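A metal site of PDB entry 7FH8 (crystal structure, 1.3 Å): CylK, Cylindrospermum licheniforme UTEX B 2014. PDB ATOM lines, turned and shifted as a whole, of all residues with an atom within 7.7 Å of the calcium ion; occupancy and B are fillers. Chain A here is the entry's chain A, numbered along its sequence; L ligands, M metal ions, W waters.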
ATOM      1  N   THR A 392     -20.403  17.697 -23.691  1.00  0.00           N
ATOM      2  CA  THR A 392     -19.932  16.333 -23.547  1.00  0.00           C
ATOM      3  C   THR A 392     -19.172  15.883 -24.781  1.00  0.00           C
ATOM      4  O   THR A 392     -19.582  16.162 -25.913  1.00  0.00           O
ATOM      5  CB  THR A 392     -21.100  15.368 -23.255  1.00  0.00           C
ATOM      6  OG1 THR A 392     -20.602  14.030 -23.120  1.00  0.00           O
ATOM      7  CG2 THR A 392     -22.171  15.398 -24.355  1.00  0.00           C
ATOM      8  N   ASN A 400     -23.060  11.348 -30.186  1.00  0.00           N
ATOM      9  CA  ASN A 400     -22.288  12.550 -30.445  1.00  0.00           C
ATOM     10  C   ASN A 400     -22.195  12.774 -31.951  1.00  0.00           C
ATOM     11  O   ASN A 400     -22.147  11.823 -32.730  1.00  0.00           O
ATOM     12  CB  ASN A 400     -20.892  12.412 -29.843  1.00  0.00           C
ATOM     13  CG  ASN A 400     -20.159  13.728 -29.731  1.00  0.00           C
ATOM     14  OD1 ASN A 400     -19.695  14.287 -30.724  1.00  0.00           O
ATOM     15  ND2 ASN A 400     -20.045  14.241 -28.510  1.00  0.00           N
ATOM     16  N   GLN A 401     -22.189  14.057 -32.361  1.00  0.00           N
ATOM     17  CA  GLN A 401     -22.103  14.373 -33.784  1.00  0.00           C
ATOM     18  C   GLN A 401     -20.791  13.865 -34.383  1.00  0.00           C
ATOM     19  O   GLN A 401     -20.726  13.611 -35.596  1.00  0.00           O
ATOM     20  CB  GLN A 401     -22.211  15.875 -34.014  1.00  0.00           C
ATOM     21  CG  GLN A 401     -23.532  16.515 -33.607  1.00  0.00           C
ATOM     22  CD  GLN A 401     -24.705  16.045 -34.443  1.00  0.00           C
ATOM     23  OE1 GLN A 401     -24.596  15.896 -35.652  1.00  0.00           O
ATOM     24  NE2 GLN A 401     -25.833  15.802 -33.784  1.00  0.00           N
ATOM     25  N   ASN A 402     -19.748  13.740 -33.575  1.00  0.00           N
ATOM     26  CA  ASN A 402     -18.431  13.251 -34.002  1.00  0.00           C
ATOM     27  C   ASN A 402     -18.179  11.976 -33.221  1.00  0.00           C
ATOM     28  O   ASN A 402     -17.637  11.991 -32.114  1.00  0.00           O
ATOM     29  CB  ASN A 402     -17.385  14.326 -33.726  1.00  0.00           C
ATOM     30  CG  ASN A 402     -16.009  13.944 -34.243  1.00  0.00           C
ATOM     31  OD1 ASN A 402     -15.874  13.054 -35.088  1.00  0.00           O
ATOM     32  ND2 ASN A 402     -14.973  14.626 -33.743  1.00  0.00           N
ATOM     33  N   PRO A 412     -11.659  14.846 -31.665  1.00  0.00           N
ATOM     34  CA  PRO A 412     -12.776  14.644 -30.737  1.00  0.00           C
ATOM     35  C   PRO A 412     -13.287  15.990 -30.237  1.00  0.00           C
ATOM     36  O   PRO A 412     -12.509  16.909 -29.967  1.00  0.00           O
ATOM     37  CB  PRO A 412     -12.151  13.847 -29.584  1.00  0.00           C
ATOM     38  CG  PRO A 412     -10.993  13.174 -30.159  1.00  0.00           C
ATOM     39  CD  PRO A 412     -10.497  14.000 -31.321  1.00  0.00           C
ATOM     40  N   SER A 413     -14.611  16.087 -30.124  1.00  0.00           N
ATOM     41  CA  SER A 413     -15.238  17.384 -29.886  1.00  0.00           C
ATOM     42  C   SER A 413     -16.510  17.231 -29.071  1.00  0.00           C
ATOM     43  O   SER A 413     -17.143  16.174 -29.027  1.00  0.00           O
ATOM     44  CB  SER A 413     -15.532  18.087 -31.221  1.00  0.00           C
ATOM     45  OG  SER A 413     -16.242  17.212 -32.083  1.00  0.00           O
ATOM     46  N   THR A 414     -16.888  18.332 -28.439  1.00  0.00           N
ATOM     47  CA  THR A 414     -18.087  18.361 -27.612  1.00  0.00           C
ATOM     48  C   THR A 414     -19.339  18.673 -28.415  1.00  0.00           C
ATOM     49  O   THR A 414     -19.303  19.347 -29.444  1.00  0.00           O
ATOM     50  CB  THR A 414     -17.969  19.410 -26.516  1.00  0.00           C
ATOM     51  OG1 THR A 414     -17.594  20.660 -27.100  1.00  0.00           O
ATOM     52  CG2 THR A 414     -16.965  18.950 -25.499  1.00  0.00           C
ATOM     53  N   ASP A 415     -20.457  18.199 -27.883  1.00  0.00           N
ATOM     54  CA  ASP A 415     -21.798  18.669 -28.203  1.00  0.00           C
ATOM     55  C   ASP A 415     -22.362  19.329 -26.947  1.00  0.00           C
ATOM     56  O   ASP A 415     -21.918  19.059 -25.825  1.00  0.00           O
ATOM     57  CB  ASP A 415     -22.711  17.487 -28.566  1.00  0.00           C
ATOM     58  CG  ASP A 415     -22.398  16.899 -29.926  1.00  0.00           C
ATOM     59  OD1 ASP A 415     -21.683  17.527 -30.744  1.00  0.00           O
ATOM     60  OD2 ASP A 415     -22.919  15.783 -30.180  1.00  0.00           O
ATOM     61  N   GLY A 416     -23.372  20.182 -27.132  1.00  0.00           N
ATOM     62  CA  GLY A 416     -24.090  20.710 -25.983  1.00  0.00           C
ATOM     63  C   GLY A 416     -25.173  19.753 -25.501  1.00  0.00           C
ATOM     64  O   GLY A 416     -25.680  18.937 -26.258  1.00  0.00           O
ATOM     65  N   GLN A 432     -29.307  16.390 -26.554  1.00  0.00           N
ATOM     66  CA  GLN A 432     -27.935  16.673 -26.979  1.00  0.00           C
ATOM     67  C   GLN A 432     -27.974  17.121 -28.430  1.00  0.00           C
ATOM     68  O   GLN A 432     -28.774  16.606 -29.214  1.00  0.00           O
ATOM     69  CB  GLN A 432     -27.038  15.425 -26.812  1.00  0.00           C
ATOM     70  CG  GLN A 432     -25.591  15.615 -27.287  1.00  0.00           C
ATOM     71  CD  GLN A 432     -24.680  14.481 -26.861  1.00  0.00           C
ATOM     72  OE1 GLN A 432     -24.912  13.828 -25.842  1.00  0.00           O
ATOM     73  NE2 GLN A 432     -23.626  14.247 -27.630  1.00  0.00           N
ATOM     74  N   PHE A 433     -27.119  18.089 -28.777  1.00  0.00           N
ATOM     75  CA  PHE A 433     -27.208  18.704 -30.095  1.00  0.00           C
ATOM     76  C   PHE A 433     -25.907  19.413 -30.424  1.00  0.00           C
ATOM     77  O   PHE A 433     -25.091  19.685 -29.541  1.00  0.00           O
ATOM     78  CB  PHE A 433     -28.389  19.673 -30.158  1.00  0.00           C
ATOM     79  CG  PHE A 433     -28.575  20.471 -28.908  1.00  0.00           C
ATOM     80  CD1 PHE A 433     -27.715  21.519 -28.624  1.00  0.00           C
ATOM     81  CD2 PHE A 433     -29.589  20.172 -28.021  1.00  0.00           C
ATOM     82  CE1 PHE A 433     -27.872  22.261 -27.457  1.00  0.00           C
ATOM     83  CE2 PHE A 433     -29.760  20.907 -26.852  1.00  0.00           C
ATOM     84  CZ  PHE A 433     -28.894  21.958 -26.581  1.00  0.00           C
ATOM     85  N   GLY A 434     -25.716  19.696 -31.704  1.00  0.00           N
ATOM     86  CA  GLY A 434     -24.564  20.480 -32.131  1.00  0.00           C
ATOM     87  C   GLY A 434     -24.135  20.110 -33.542  1.00  0.00           C
ATOM     88  O   GLY A 434     -24.950  19.709 -34.363  1.00  0.00           O
ATOM     89  N   THR A 435     -22.842  20.275 -33.787  1.00  0.00           N
ATOM     90  CA  THR A 435     -22.186  20.038 -35.073  1.00  0.00           C
ATOM     91  C   THR A 435     -21.051  19.033 -34.872  1.00  0.00           C
ATOM     92  O   THR A 435     -20.756  18.628 -33.750  1.00  0.00           O
ATOM     93  CB  THR A 435     -21.562  21.326 -35.625  1.00  0.00           C
ATOM     94  OG1 THR A 435     -20.473  21.724 -34.793  1.00  0.00           O
ATOM     95  CG2 THR A 435     -22.589  22.453 -35.691  1.00  0.00           C
ATOM     96  N   ILE A 436     -20.394  18.661 -35.977  1.00  0.00           N
ATOM     97  CA  ILE A 436     -19.261  17.739 -35.876  1.00  0.00           C
ATOM     98  C   ILE A 436     -18.090  18.338 -35.101  1.00  0.00           C
ATOM     99  O   ILE A 436     -17.218  17.595 -34.627  1.00  0.00           O
ATOM    100  CB  ILE A 436     -18.820  17.265 -37.278  1.00  0.00           C
ATOM    101  CG1 ILE A 436     -18.018  15.972 -37.182  1.00  0.00           C
ATOM    102  CG2 ILE A 436     -18.025  18.348 -37.966  1.00  0.00           C
ATOM    103  CD1 ILE A 436     -17.678  15.365 -38.528  1.00  0.00           C
ATOM    104  N   THR A 437     -18.023  19.658 -34.968  1.00  0.00           N
ATOM    105  CA  THR A 437     -16.899  20.299 -34.309  1.00  0.00           C
ATOM    106  C   THR A 437     -17.293  20.732 -32.891  1.00  0.00           C
ATOM    107  O   THR A 437     -18.266  20.218 -32.323  1.00  0.00           O
ATOM    108  CB  THR A 437     -16.314  21.391 -35.220  1.00  0.00           C
ATOM    109  OG1 THR A 437     -15.134  21.963 -34.614  1.00  0.00           O
ATOM    110  CG2 THR A 437     -17.348  22.490 -35.498  1.00  0.00           C
ATOM    111  N   LEU A 438     -16.524  21.650 -32.305  1.00  0.00           N
ATOM    112  CA  LEU A 438     -16.763  22.133 -30.953  1.00  0.00           C
ATOM    113  C   LEU A 438     -18.102  22.850 -30.842  1.00  0.00           C
ATOM    114  O   LEU A 438     -18.369  23.811 -31.578  1.00  0.00           O
ATOM    115  CB  LEU A 438     -15.620  23.080 -30.559  1.00  0.00           C
ATOM    116  CG  LEU A 438     -15.611  23.753 -29.172  1.00  0.00           C
ATOM    117  CD1 LEU A 438     -14.195  24.185 -28.881  1.00  0.00           C
ATOM    118  CD2 LEU A 438     -16.532  24.974 -29.094  1.00  0.00           C
ATOM    119  N   ASP A 439     -18.936  22.395 -29.906  1.00  0.00           N
ATOM    120  CA  ASP A 439     -20.104  23.147 -29.442  1.00  0.00           C
ATOM    121  C   ASP A 439     -20.102  23.046 -27.920  1.00  0.00           C
ATOM    122  O   ASP A 439     -20.187  21.942 -27.369  1.00  0.00           O
ATOM    123  CB  ASP A 439     -21.425  22.564 -29.977  1.00  0.00           C
ATOM    124  CG  ASP A 439     -21.304  22.044 -31.384  1.00  0.00           C
ATOM    125  OD1 ASP A 439     -21.248  22.849 -32.346  1.00  0.00           O
ATOM    126  OD2 ASP A 439     -21.330  20.808 -31.549  1.00  0.00           O
ATOM    127  N   ASP A 440     -19.989  24.172 -27.236  1.00  0.00           N
ATOM    128  CA  ASP A 440     -19.948  24.277 -25.786  1.00  0.00           C
ATOM    129  C   ASP A 440     -21.226  24.956 -25.289  1.00  0.00           C
ATOM    130  O   ASP A 440     -21.860  25.701 -26.045  1.00  0.00           O
ATOM    131  CB  ASP A 440     -18.755  25.151 -25.357  1.00  0.00           C
ATOM    132  CG  ASP A 440     -17.409  24.463 -25.528  1.00  0.00           C
ATOM    133  OD1 ASP A 440     -17.381  23.221 -25.721  1.00  0.00           O
ATOM    134  OD2 ASP A 440     -16.384  25.170 -25.483  1.00  0.00           O
ATOM    135  N   THR A 458     -19.959  27.827 -30.802  1.00  0.00           N
ATOM    136  CA  THR A 458     -19.673  26.780 -31.758  1.00  0.00           C
ATOM    137  C   THR A 458     -18.597  27.231 -32.733  1.00  0.00           C
ATOM    138  O   THR A 458     -18.550  28.411 -33.109  1.00  0.00           O
ATOM    139  CB  THR A 458     -20.929  26.320 -32.538  1.00  0.00           C
ATOM    140  OG1 THR A 458     -20.576  25.247 -33.415  1.00  0.00           O
ATOM    141  CG2 THR A 458     -21.550  27.457 -33.357  1.00  0.00           C
HETATM  142  C1  LIG L   1      -7.289  18.241 -27.734  1.00  0.00           C
HETATM  143  C2  LIG L   1      -9.455  17.364 -26.573  1.00  0.00           C
HETATM  144  C3  LIG L   1     -10.822  19.326 -27.414  1.00  0.00           C
HETATM  145  C4  LIG L   1     -13.022  22.867 -25.006  1.00  0.00           C
HETATM  146  C5  LIG L   1     -14.355  22.651 -25.595  1.00  0.00           C
HETATM  147  C6  LIG L   1     -14.914  21.414 -25.080  1.00  0.00           C
HETATM  148  C7  LIG L   1     -10.952  23.926 -25.842  1.00  0.00           C
HETATM  149  C8  LIG L   1      -9.895  23.802 -28.130  1.00  0.00           C
HETATM  150  C9  LIG L   1      -8.698  23.211 -30.270  1.00  0.00           C
HETATM  151  C10 LIG L   1       1.310  21.192 -26.023  1.00  0.00           C
HETATM  152  C11 LIG L   1       0.096  22.063 -26.327  1.00  0.00           C
HETATM  153  C12 LIG L   1      -1.126  21.271 -26.782  1.00  0.00           C
HETATM  154  C13 LIG L   1      -2.170  22.150 -27.458  1.00  0.00           C
HETATM  155  C14 LIG L   1      -3.157  21.327 -28.300  1.00  0.00           C
HETATM  156  C15 LIG L   1      -4.218  20.685 -27.406  1.00  0.00           C
HETATM  157  C16 LIG L   1      -5.274  19.860 -28.143  1.00  0.00           C
HETATM  158  C17 LIG L   1      -6.129  19.047 -27.132  1.00  0.00           C
HETATM  159  C18 LIG L   1      -7.911  17.252 -26.697  1.00  0.00           C
HETATM  160  C19 LIG L   1      -7.552  15.845 -27.100  1.00  0.00           C
HETATM  161  C20 LIG L   1     -10.077  18.742 -26.403  1.00  0.00           C
HETATM  162  C21 LIG L   1     -11.404  20.590 -27.280  1.00  0.00           C
HETATM  163  C22 LIG L   1     -11.293  21.378 -26.133  1.00  0.00           C
HETATM  164  C23 LIG L   1     -11.949  22.785 -26.068  1.00  0.00           C
HETATM  165  C24 LIG L   1     -15.185  21.501 -23.596  1.00  0.00           C
HETATM  166  C25 LIG L   1      -9.664  23.779 -26.629  1.00  0.00           C
HETATM  167  C26 LIG L   1      -8.603  23.875 -28.915  1.00  0.00           C
HETATM  168  C27 LIG L   1      -7.354  23.232 -30.947  1.00  0.00           C
HETATM  169  C28 LIG L   1      -9.727  23.882 -31.213  1.00  0.00           C
HETATM  170  C29 LIG L   1     -10.347  22.956 -32.195  1.00  0.00           C
HETATM  171  C30 LIG L   1      -9.767  22.772 -33.453  1.00  0.00           C
HETATM  172  C31 LIG L   1     -10.329  21.899 -34.368  1.00  0.00           C
HETATM  173  C32 LIG L   1     -11.471  21.158 -34.081  1.00  0.00           C
HETATM  174  C33 LIG L   1     -12.031  21.339 -32.810  1.00  0.00           C
HETATM  175  C34 LIG L   1     -11.477  22.221 -31.873  1.00  0.00           C
HETATM  176  C35 LIG L   1     -10.529  20.776 -25.103  1.00  0.00           C
HETATM  177  C36 LIG L   1      -9.941  19.504 -25.221  1.00  0.00           C
HETATM  178  F1  LIG L   1      -2.432  20.349 -28.918  1.00  0.00           F
HETATM  179  O1  LIG L   1     -12.119  21.061 -28.347  1.00  0.00           O
HETATM  180  O2  LIG L   1      -9.710  21.797 -35.583  1.00  0.00           O
HETATM  181  O3  LIG L   1     -13.140  20.658 -32.440  1.00  0.00           O
HETATM  182  O4  LIG L   1     -10.389  21.502 -23.957  1.00  0.00           O
HETATM  183 CA    CA M   1     -20.057  18.917 -31.607  1.00  0.00          CA
HETATM  184  O   HOH W   1     -18.891  16.870 -31.571  1.00  0.00           O
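Water W1 lies within hydrogen-bond range of OG of Ser 413 (2.7 Å) and OD1 of Asn 400 (2.8 Å).
The calcium ion is bound by O of Thr 435 (2.3 Å), OD2 of Asp 439 (2.3 Å), OD1 of Asp 415 (2.3 Å), O of Thr 437 (2.3 Å), O of Thr 414 (2.3 Å) and water W1 (2.4 Å).
OG1 of Thr 437 sits at hydrogen-bond distance from O3 of the ligand (3.2 Å).
The side-chain hydroxyl (OG1) of Thr 435 sits close to the backbone NH (N) of Thr 437, 3.2 Å away.
OD1 of Asp 439 sits at hydrogen-bond distance from OG1 of Thr 458 (2.7 Å).
The side-chain carboxylate (OD2) of Asp 415 sits at hydrogen-bond distance from the backbone NH (N) of Gln 401 (2.9 Å).
O of Asp 415 is in hydrogen-bond range of N of Thr 392, at 3.0 Å.
The side-chain carboxylate of Asp 415 sits at hydrogen-bond distance from the side-chain amide nitrogen of Gln 432 (3.1 Å).
The side-chain hydroxyl (OG1) of Thr 414 sits at hydrogen-bond distance from the side-chain carboxylate (OD1) of Asp 440.
Five residues have an atom within 4 Å of the calcium ion: Thr 414, Asp 415, Thr 435, Thr 437 and Asp 439.
Along chain A the residues within 4 Å of the calcium ion span positions 414 to 439.
The nearest printed residue that does not touch the calcium ion is Ile 436 (4.1 Å).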
